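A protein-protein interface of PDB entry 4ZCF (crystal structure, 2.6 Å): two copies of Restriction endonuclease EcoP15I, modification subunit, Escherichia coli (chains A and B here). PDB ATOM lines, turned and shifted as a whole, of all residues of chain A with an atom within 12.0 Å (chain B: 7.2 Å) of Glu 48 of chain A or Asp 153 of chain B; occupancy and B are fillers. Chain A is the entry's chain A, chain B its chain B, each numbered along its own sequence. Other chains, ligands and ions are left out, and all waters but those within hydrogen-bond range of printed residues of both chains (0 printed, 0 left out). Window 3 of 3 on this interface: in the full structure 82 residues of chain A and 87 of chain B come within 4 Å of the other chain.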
ATOM      1  N   LEU A  41       7.681  34.227 -30.737  1.00  0.00           N
ATOM      2  CA  LEU A  41       8.308  33.164 -31.536  1.00  0.00           C
ATOM      3  C   LEU A  41       7.813  31.770 -31.149  1.00  0.00           C
ATOM      4  O   LEU A  41       7.526  30.978 -32.040  1.00  0.00           O
ATOM      5  CB  LEU A  41       9.848  33.230 -31.524  1.00  0.00           C
ATOM      6  CG  LEU A  41      10.510  34.439 -32.220  1.00  0.00           C
ATOM      7  CD1 LEU A  41      11.985  34.536 -31.849  1.00  0.00           C
ATOM      8  CD2 LEU A  41      10.382  34.360 -33.741  1.00  0.00           C
ATOM      9  N   GLU A  42       7.644  31.486 -29.840  1.00  0.00           N
ATOM     10  CA  GLU A  42       7.116  30.186 -29.404  1.00  0.00           C
ATOM     11  C   GLU A  42       5.653  29.968 -29.833  1.00  0.00           C
ATOM     12  O   GLU A  42       5.266  28.821 -30.078  1.00  0.00           O
ATOM     13  CB  GLU A  42       7.401  29.872 -27.916  1.00  0.00           C
ATOM     14  CG  GLU A  42       6.691  30.766 -26.908  1.00  0.00           C
ATOM     15  CD  GLU A  42       7.149  30.654 -25.465  1.00  0.00           C
ATOM     16  OE1 GLU A  42       8.374  30.754 -25.213  1.00  0.00           O
ATOM     17  OE2 GLU A  42       6.273  30.535 -24.577  1.00  0.00           O
ATOM     18  N   ILE A  43       4.878  31.073 -30.018  1.00  0.00           N
ATOM     19  CA  ILE A  43       3.483  31.055 -30.504  1.00  0.00           C
ATOM     20  C   ILE A  43       3.469  30.688 -31.999  1.00  0.00           C
ATOM     21  O   ILE A  43       2.710  29.806 -32.417  1.00  0.00           O
ATOM     22  CB  ILE A  43       2.719  32.383 -30.193  1.00  0.00           C
ATOM     23  CG1 ILE A  43       2.407  32.500 -28.670  1.00  0.00           C
ATOM     24  CG2 ILE A  43       1.435  32.530 -31.054  1.00  0.00           C
ATOM     25  CD1 ILE A  43       2.050  33.861 -28.160  1.00  0.00           C
ATOM     26  N   ILE A  44       4.338  31.337 -32.789  1.00  0.00           N
ATOM     27  CA  ILE A  44       4.482  31.080 -34.222  1.00  0.00           C
ATOM     28  C   ILE A  44       4.835  29.590 -34.546  1.00  0.00           C
ATOM     29  O   ILE A  44       4.437  29.094 -35.604  1.00  0.00           O
ATOM     30  CB  ILE A  44       5.429  32.126 -34.858  1.00  0.00           C
ATOM     31  CG1 ILE A  44       4.791  33.524 -34.800  1.00  0.00           C
ATOM     32  CG2 ILE A  44       5.815  31.753 -36.299  1.00  0.00           C
ATOM     33  CD1 ILE A  44       5.764  34.671 -34.903  1.00  0.00           C
ATOM     34  N   ARG A  45       5.509  28.875 -33.610  1.00  0.00           N
ATOM     35  CA  ARG A  45       5.908  27.464 -33.759  1.00  0.00           C
ATOM     36  C   ARG A  45       4.847  26.465 -33.254  1.00  0.00           C
ATOM     37  O   ARG A  45       4.558  26.403 -32.053  1.00  0.00           O
ATOM     38  CB  ARG A  45       7.276  27.189 -33.102  1.00  0.00           C
ATOM     39  CG  ARG A  45       8.392  28.168 -33.494  1.00  0.00           C
ATOM     40  CD  ARG A  45       9.740  27.828 -32.870  1.00  0.00           C
ATOM     41  NE  ARG A  45       9.667  27.577 -31.426  1.00  0.00           N
ATOM     42  CZ  ARG A  45      10.200  28.357 -30.489  1.00  0.00           C
ATOM     43  NH1 ARG A  45      10.863  29.458 -30.827  1.00  0.00           N
ATOM     44  NH2 ARG A  45      10.081  28.037 -29.205  1.00  0.00           N
ATOM     45  N   ALA A  46       4.277  25.682 -34.190  1.00  0.00           N
ATOM     46  CA  ALA A  46       3.253  24.654 -33.951  1.00  0.00           C
ATOM     47  C   ALA A  46       3.784  23.260 -34.383  1.00  0.00           C
ATOM     48  O   ALA A  46       3.094  22.511 -35.086  1.00  0.00           O
ATOM     49  CB  ALA A  46       1.981  25.006 -34.722  1.00  0.00           C
ATOM     50  N   SER A  47       5.020  22.926 -33.955  1.00  0.00           N
ATOM     51  CA  SER A  47       5.690  21.672 -34.291  1.00  0.00           C
ATOM     52  C   SER A  47       6.021  20.776 -33.078  1.00  0.00           C
ATOM     53  O   SER A  47       6.265  21.279 -31.979  1.00  0.00           O
ATOM     54  CB  SER A  47       6.945  21.959 -35.107  1.00  0.00           C
ATOM     55  N   GLU A  48       6.037  19.441 -33.301  1.00  0.00           N
ATOM     56  CA  GLU A  48       6.343  18.418 -32.293  1.00  0.00           C
ATOM     57  C   GLU A  48       7.755  17.847 -32.475  1.00  0.00           C
ATOM     58  O   GLU A  48       8.695  18.568 -32.813  1.00  0.00           O
ATOM     59  CB  GLU A  48       5.318  17.296 -32.362  1.00  0.00           C
ATOM     60  N   LYS A  53       8.875  18.292 -23.314  1.00  0.00           N
ATOM     61  CA  LYS A  53       7.757  17.692 -22.574  1.00  0.00           C
ATOM     62  C   LYS A  53       7.194  18.656 -21.516  1.00  0.00           C
ATOM     63  O   LYS A  53       7.938  19.169 -20.696  1.00  0.00           O
ATOM     64  CB  LYS A  53       8.172  16.361 -21.944  1.00  0.00           C
ATOM     65  N   GLU A  54       5.887  18.934 -21.591  1.00  0.00           N
ATOM     66  CA  GLU A  54       5.123  19.813 -20.707  1.00  0.00           C
ATOM     67  C   GLU A  54       5.058  19.261 -19.271  1.00  0.00           C
ATOM     68  O   GLU A  54       4.654  18.109 -19.068  1.00  0.00           O
ATOM     69  CB  GLU A  54       3.710  19.905 -21.259  1.00  0.00           C
ATOM     70  CG  GLU A  54       3.140  21.296 -21.347  1.00  0.00           C
ATOM     71  CD  GLU A  54       1.850  21.284 -22.132  1.00  0.00           C
ATOM     72  OE1 GLU A  54       0.965  20.451 -21.818  1.00  0.00           O
ATOM     73  OE2 GLU A  54       1.753  22.068 -23.104  1.00  0.00           O
ATOM     74  N   SER A  55       5.456  20.080 -18.274  1.00  0.00           N
ATOM     75  CA  SER A  55       5.438  19.712 -16.860  1.00  0.00           C
ATOM     76  C   SER A  55       5.236  20.937 -15.971  1.00  0.00           C
ATOM     77  O   SER A  55       5.406  22.064 -16.440  1.00  0.00           O
ATOM     78  CB  SER A  55       6.704  18.953 -16.469  1.00  0.00           C
ATOM     79  OG  SER A  55       7.855  19.779 -16.440  1.00  0.00           O
ATOM     80  N   PRO B 143      -6.330  10.587 -28.771  1.00  0.00           N
ATOM     81  CA  PRO B 143      -4.951  11.107 -28.614  1.00  0.00           C
ATOM     82  C   PRO B 143      -4.369  11.675 -29.907  1.00  0.00           C
ATOM     83  O   PRO B 143      -3.572  12.609 -29.858  1.00  0.00           O
ATOM     84  CB  PRO B 143      -4.157   9.886 -28.142  1.00  0.00           C
ATOM     85  CG  PRO B 143      -5.169   8.971 -27.558  1.00  0.00           C
ATOM     86  CD  PRO B 143      -6.408   9.166 -28.381  1.00  0.00           C
ATOM     87  N   LEU B 146      -5.861  15.267 -30.351  1.00  0.00           N
ATOM     88  CA  LEU B 146      -5.104  16.177 -29.491  1.00  0.00           C
ATOM     89  C   LEU B 146      -3.691  16.433 -30.028  1.00  0.00           C
ATOM     90  O   LEU B 146      -3.254  17.583 -30.051  1.00  0.00           O
ATOM     91  CB  LEU B 146      -5.077  15.711 -28.024  1.00  0.00           C
ATOM     92  CG  LEU B 146      -4.442  16.700 -27.028  1.00  0.00           C
ATOM     93  CD1 LEU B 146      -5.309  17.932 -26.826  1.00  0.00           C
ATOM     94  CD2 LEU B 146      -4.154  16.044 -25.725  1.00  0.00           C
ATOM     95  N   SER B 147      -3.006  15.378 -30.491  1.00  0.00           N
ATOM     96  CA  SER B 147      -1.671  15.460 -31.083  1.00  0.00           C
ATOM     97  C   SER B 147      -1.613  16.513 -32.217  1.00  0.00           C
ATOM     98  O   SER B 147      -0.703  17.336 -32.225  1.00  0.00           O
ATOM     99  CB  SER B 147      -1.244  14.090 -31.608  1.00  0.00           C
ATOM    100  OG  SER B 147       0.135  14.020 -31.927  1.00  0.00           O
ATOM    101  N   GLU B 148      -2.594  16.516 -33.141  1.00  0.00           N
ATOM    102  CA  GLU B 148      -2.624  17.479 -34.254  1.00  0.00           C
ATOM    103  C   GLU B 148      -3.079  18.881 -33.824  1.00  0.00           C
ATOM    104  O   GLU B 148      -2.451  19.876 -34.197  1.00  0.00           O
ATOM    105  CB  GLU B 148      -3.500  16.958 -35.389  1.00  0.00           C
ATOM    106  N   ALA B 150      -3.002  20.194 -30.794  1.00  0.00           N
ATOM    107  CA  ALA B 150      -2.115  20.707 -29.736  1.00  0.00           C
ATOM    108  C   ALA B 150      -0.884  21.571 -30.059  1.00  0.00           C
ATOM    109  O   ALA B 150      -0.530  22.412 -29.275  1.00  0.00           O
ATOM    110  CB  ALA B 150      -1.757  19.609 -28.769  1.00  0.00           C
ATOM    111  N   GLY B 151      -0.185  21.350 -31.157  1.00  0.00           N
ATOM    112  CA  GLY B 151       0.308  20.065 -31.536  1.00  0.00           C
ATOM    113  C   GLY B 151       1.511  19.628 -30.776  1.00  0.00           C
ATOM    114  O   GLY B 151       2.543  20.241 -30.724  1.00  0.00           O
ATOM    115  N   ILE B 152       1.313  18.465 -30.224  1.00  0.00           N
ATOM    116  CA  ILE B 152       2.265  17.680 -29.446  1.00  0.00           C
ATOM    117  C   ILE B 152       2.385  16.265 -30.055  1.00  0.00           C
ATOM    118  O   ILE B 152       1.679  15.963 -31.013  1.00  0.00           O
ATOM    119  CB  ILE B 152       1.757  17.660 -27.972  1.00  0.00           C
ATOM    120  CG1 ILE B 152       0.282  17.148 -27.883  1.00  0.00           C
ATOM    121  CG2 ILE B 152       1.930  19.039 -27.330  1.00  0.00           C
ATOM    122  CD1 ILE B 152      -0.417  17.260 -26.578  1.00  0.00           C
ATOM    123  N   ASP B 153       3.257  15.396 -29.514  1.00  0.00           N
ATOM    124  CA  ASP B 153       3.363  14.031 -30.040  1.00  0.00           C
ATOM    125  C   ASP B 153       2.227  13.166 -29.469  1.00  0.00           C
ATOM    126  O   ASP B 153       1.528  13.620 -28.559  1.00  0.00           O
ATOM    127  CB  ASP B 153       4.759  13.422 -29.781  1.00  0.00           C
ATOM    128  CG  ASP B 153       5.074  13.147 -28.325  1.00  0.00           C
ATOM    129  OD1 ASP B 153       4.655  12.091 -27.821  1.00  0.00           O
ATOM    130  OD2 ASP B 153       5.783  13.964 -27.709  1.00  0.00           O
ATOM    131  N   LEU B 154       2.046  11.931 -30.004  1.00  0.00           N
ATOM    132  CA  LEU B 154       1.013  10.981 -29.567  1.00  0.00           C
ATOM    133  C   LEU B 154       1.174  10.591 -28.089  1.00  0.00           C
ATOM    134  O   LEU B 154       0.178  10.566 -27.368  1.00  0.00           O
ATOM    135  CB  LEU B 154       1.018   9.735 -30.454  1.00  0.00           C
ATOM    136  N   ASP B 155       2.414  10.325 -27.634  1.00  0.00           N
ATOM    137  CA  ASP B 155       2.692   9.953 -26.245  1.00  0.00           C
ATOM    138  C   ASP B 155       2.407  11.107 -25.268  1.00  0.00           C
ATOM    139  O   ASP B 155       1.791  10.872 -24.219  1.00  0.00           O
ATOM    140  CB  ASP B 155       4.121   9.395 -26.087  1.00  0.00           C
ATOM    141  CG  ASP B 155       4.372   8.099 -26.846  1.00  0.00           C
ATOM    142  OD1 ASP B 155       3.497   7.196 -26.800  1.00  0.00           O
ATOM    143  OD2 ASP B 155       5.456   7.976 -27.462  1.00  0.00           O
ATOM    144  N   GLU B 156       2.817  12.349 -25.636  1.00  0.00           N
ATOM    145  CA  GLU B 156       2.562  13.580 -24.869  1.00  0.00           C
ATOM    146  C   GLU B 156       1.045  13.829 -24.833  1.00  0.00           C
ATOM    147  O   GLU B 156       0.499  14.143 -23.769  1.00  0.00           O
ATOM    148  CB  GLU B 156       3.313  14.790 -25.478  1.00  0.00           C
ATOM    149  CG  GLU B 156       3.034  16.126 -24.792  1.00  0.00           C
ATOM    150  CD  GLU B 156       4.082  16.667 -23.838  1.00  0.00           C
ATOM    151  OE1 GLU B 156       4.583  15.890 -22.993  1.00  0.00           O
ATOM    152  OE2 GLU B 156       4.370  17.885 -23.906  1.00  0.00           O
ATOM    153  N   ALA B 157       0.371  13.634 -25.997  1.00  0.00           N
ATOM    154  CA  ALA B 157      -1.075  13.761 -26.141  1.00  0.00           C
ATOM    155  C   ALA B 157      -1.806  12.759 -25.256  1.00  0.00           C
ATOM    156  O   ALA B 157      -2.782  13.142 -24.620  1.00  0.00           O
ATOM    157  CB  ALA B 157      -1.475  13.583 -27.586  1.00  0.00           C
ATOM    158  N   LYS B 158      -1.311  11.496 -25.179  1.00  0.00           N
ATOM    159  CA  LYS B 158      -1.896  10.433 -24.351  1.00  0.00           C
ATOM    160  C   LYS B 158      -1.790  10.781 -22.867  1.00  0.00           C
ATOM    161  O   LYS B 158      -2.766  10.599 -22.134  1.00  0.00           O
ATOM    162  CB  LYS B 158      -1.222   9.076 -24.617  1.00  0.00           C
ATOM    163  CG  LYS B 158      -1.738   8.355 -25.855  1.00  0.00           C
ATOM    164  CD  LYS B 158      -0.956   7.071 -26.136  1.00  0.00           C
ATOM    165  CE  LYS B 158      -1.236   6.541 -27.521  1.00  0.00           C
ATOM    166  NZ  LYS B 158      -0.426   5.330 -27.807  1.00  0.00           N
ATOM    167  N   ARG B 159      -0.599  11.295 -22.441  1.00  0.00           N
ATOM    168  CA  ARG B 159      -0.291  11.723 -21.075  1.00  0.00           C
ATOM    169  C   ARG B 159      -1.290  12.790 -20.577  1.00  0.00           C
ATOM    170  O   ARG B 159      -1.770  12.698 -19.435  1.00  0.00           O
ATOM    171  CB  ARG B 159       1.171  12.224 -20.983  1.00  0.00           C
ATOM    172  CG  ARG B 159       1.482  13.046 -19.720  1.00  0.00           C
ATOM    173  CD  ARG B 159       2.929  12.951 -19.310  1.00  0.00           C
ATOM    174  NE  ARG B 159       3.784  13.902 -20.021  1.00  0.00           N
ATOM    175  CZ  ARG B 159       4.347  14.970 -19.464  1.00  0.00           C
ATOM    176  NH1 ARG B 159       4.149  15.242 -18.179  1.00  0.00           N
ATOM    177  NH2 ARG B 159       5.118  15.770 -20.186  1.00  0.00           N
ATOM    178  N   ILE B 160      -1.600  13.781 -21.457  1.00  0.00           N
ATOM    179  CA  ILE B 160      -2.514  14.893 -21.182  1.00  0.00           C
ATOM    180  C   ILE B 160      -3.968  14.466 -20.995  1.00  0.00           C
ATOM    181  O   ILE B 160      -4.630  14.974 -20.085  1.00  0.00           O
ATOM    182  CB  ILE B 160      -2.281  16.112 -22.128  1.00  0.00           C
ATOM    183  CG1 ILE B 160      -0.990  16.852 -21.721  1.00  0.00           C
ATOM    184  CG2 ILE B 160      -3.466  17.096 -22.157  1.00  0.00           C
ATOM    185  CD1 ILE B 160      -0.179  17.389 -22.879  1.00  0.00           C
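OE1 of Glu 156 of chain B lies within salt-bridge range of NH2 of Arg 159 of chain B. OG of Ser 147 of chain B is in hydrogen-bond range of O of Ile 152 of chain B, 2.6 Å away. The backbone NH (N) of Glu 156 of chain B is in hydrogen-bond range of the side-chain carboxylate (OD1) of Asp 153 of chain B (2.9 Å). OD1 of Asp 153 of chain B is in hydrogen-bond range of N of Asp 155 of chain B.
Glu 42 of chain A touches none of the printed residues of chain B. Ser 47 of chain A touches none of the printed residues of chain B. Of the printed residues of chain B, Glu 48 of chain A touches Ile 152 (3.9 Å) and Asp 153 (3.996 Å). Printed residues of chain B within 4 Å of Lys 53 of chain A: Glu 156 and Arg 159. Of the printed residues of chain B, Glu 54 of chain A touches Glu 156, Arg 159 and Ile 160. No residue of chain A comes within 4 Å of Ser 147 of chain B. No residue of chain A comes within 4 Å of Gly 151 of chain B. Ile 152 of chain B touches just one residue of chain A: Glu 48. Of the printed residues of chain A, Asp 153 of chain B touches Glu 48 (3.996 Å). Leu 154 of chain B touches none of the printed residues of chain A. No residue of chain A comes within 4 Å of Asp 155 of chain B. Glu 156 of chain B touches just these residues of chain A: Lys 53 (3.6 Å) and Glu 54 (3.0 Å). No residue of chain A comes within 4 Å of Ala 157 of chain B. Printed residues of chain A within 4 Å of Arg 159 of chain B: Lys 53 and Glu 54. Printed residues of chain A within 4 Å of Ile 160 of chain B: Glu 54 (3.4 Å). The nearest printed residue of chain B that does not touch Glu 48 of chain A is Gly 151 of chain B (4.4 Å). The nearest printed residue of chain B that does not touch Glu 54 of chain A is Ile 152 of chain B (5.2 Å).
Among the printed residues, no Asp or Glu carboxylate lies within 4 Å of a Lys or Arg side-chain nitrogen of the other chain.
Ile 152 of chain B touches Glu 48 of chain A (C to CB, 3.9 Å). CB of Glu 48 of chain A touches N of Asp 153 of chain B, 3.996 Å away. Glu 156 of chain B touches Lys 53 of chain A (OE2 to CA, 3.6 Å). Arg 159 of chain B touches Lys 53 of chain A (NH2 to CB, 3.6 Å). Ile 160 of chain B touches Glu 54 of chain A.
The side-chain carboxylate of Glu 156 of chain B lies within hydrogen-bond range of the backbone NH of Glu 54 of chain A (3.0 Å). The backbone carbonyl oxygen of Glu 54 of chain A sits at hydrogen-bond distance from the guanidinium group of Arg 159 of chain B (2.6 Å).
No position is printed for both chains.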
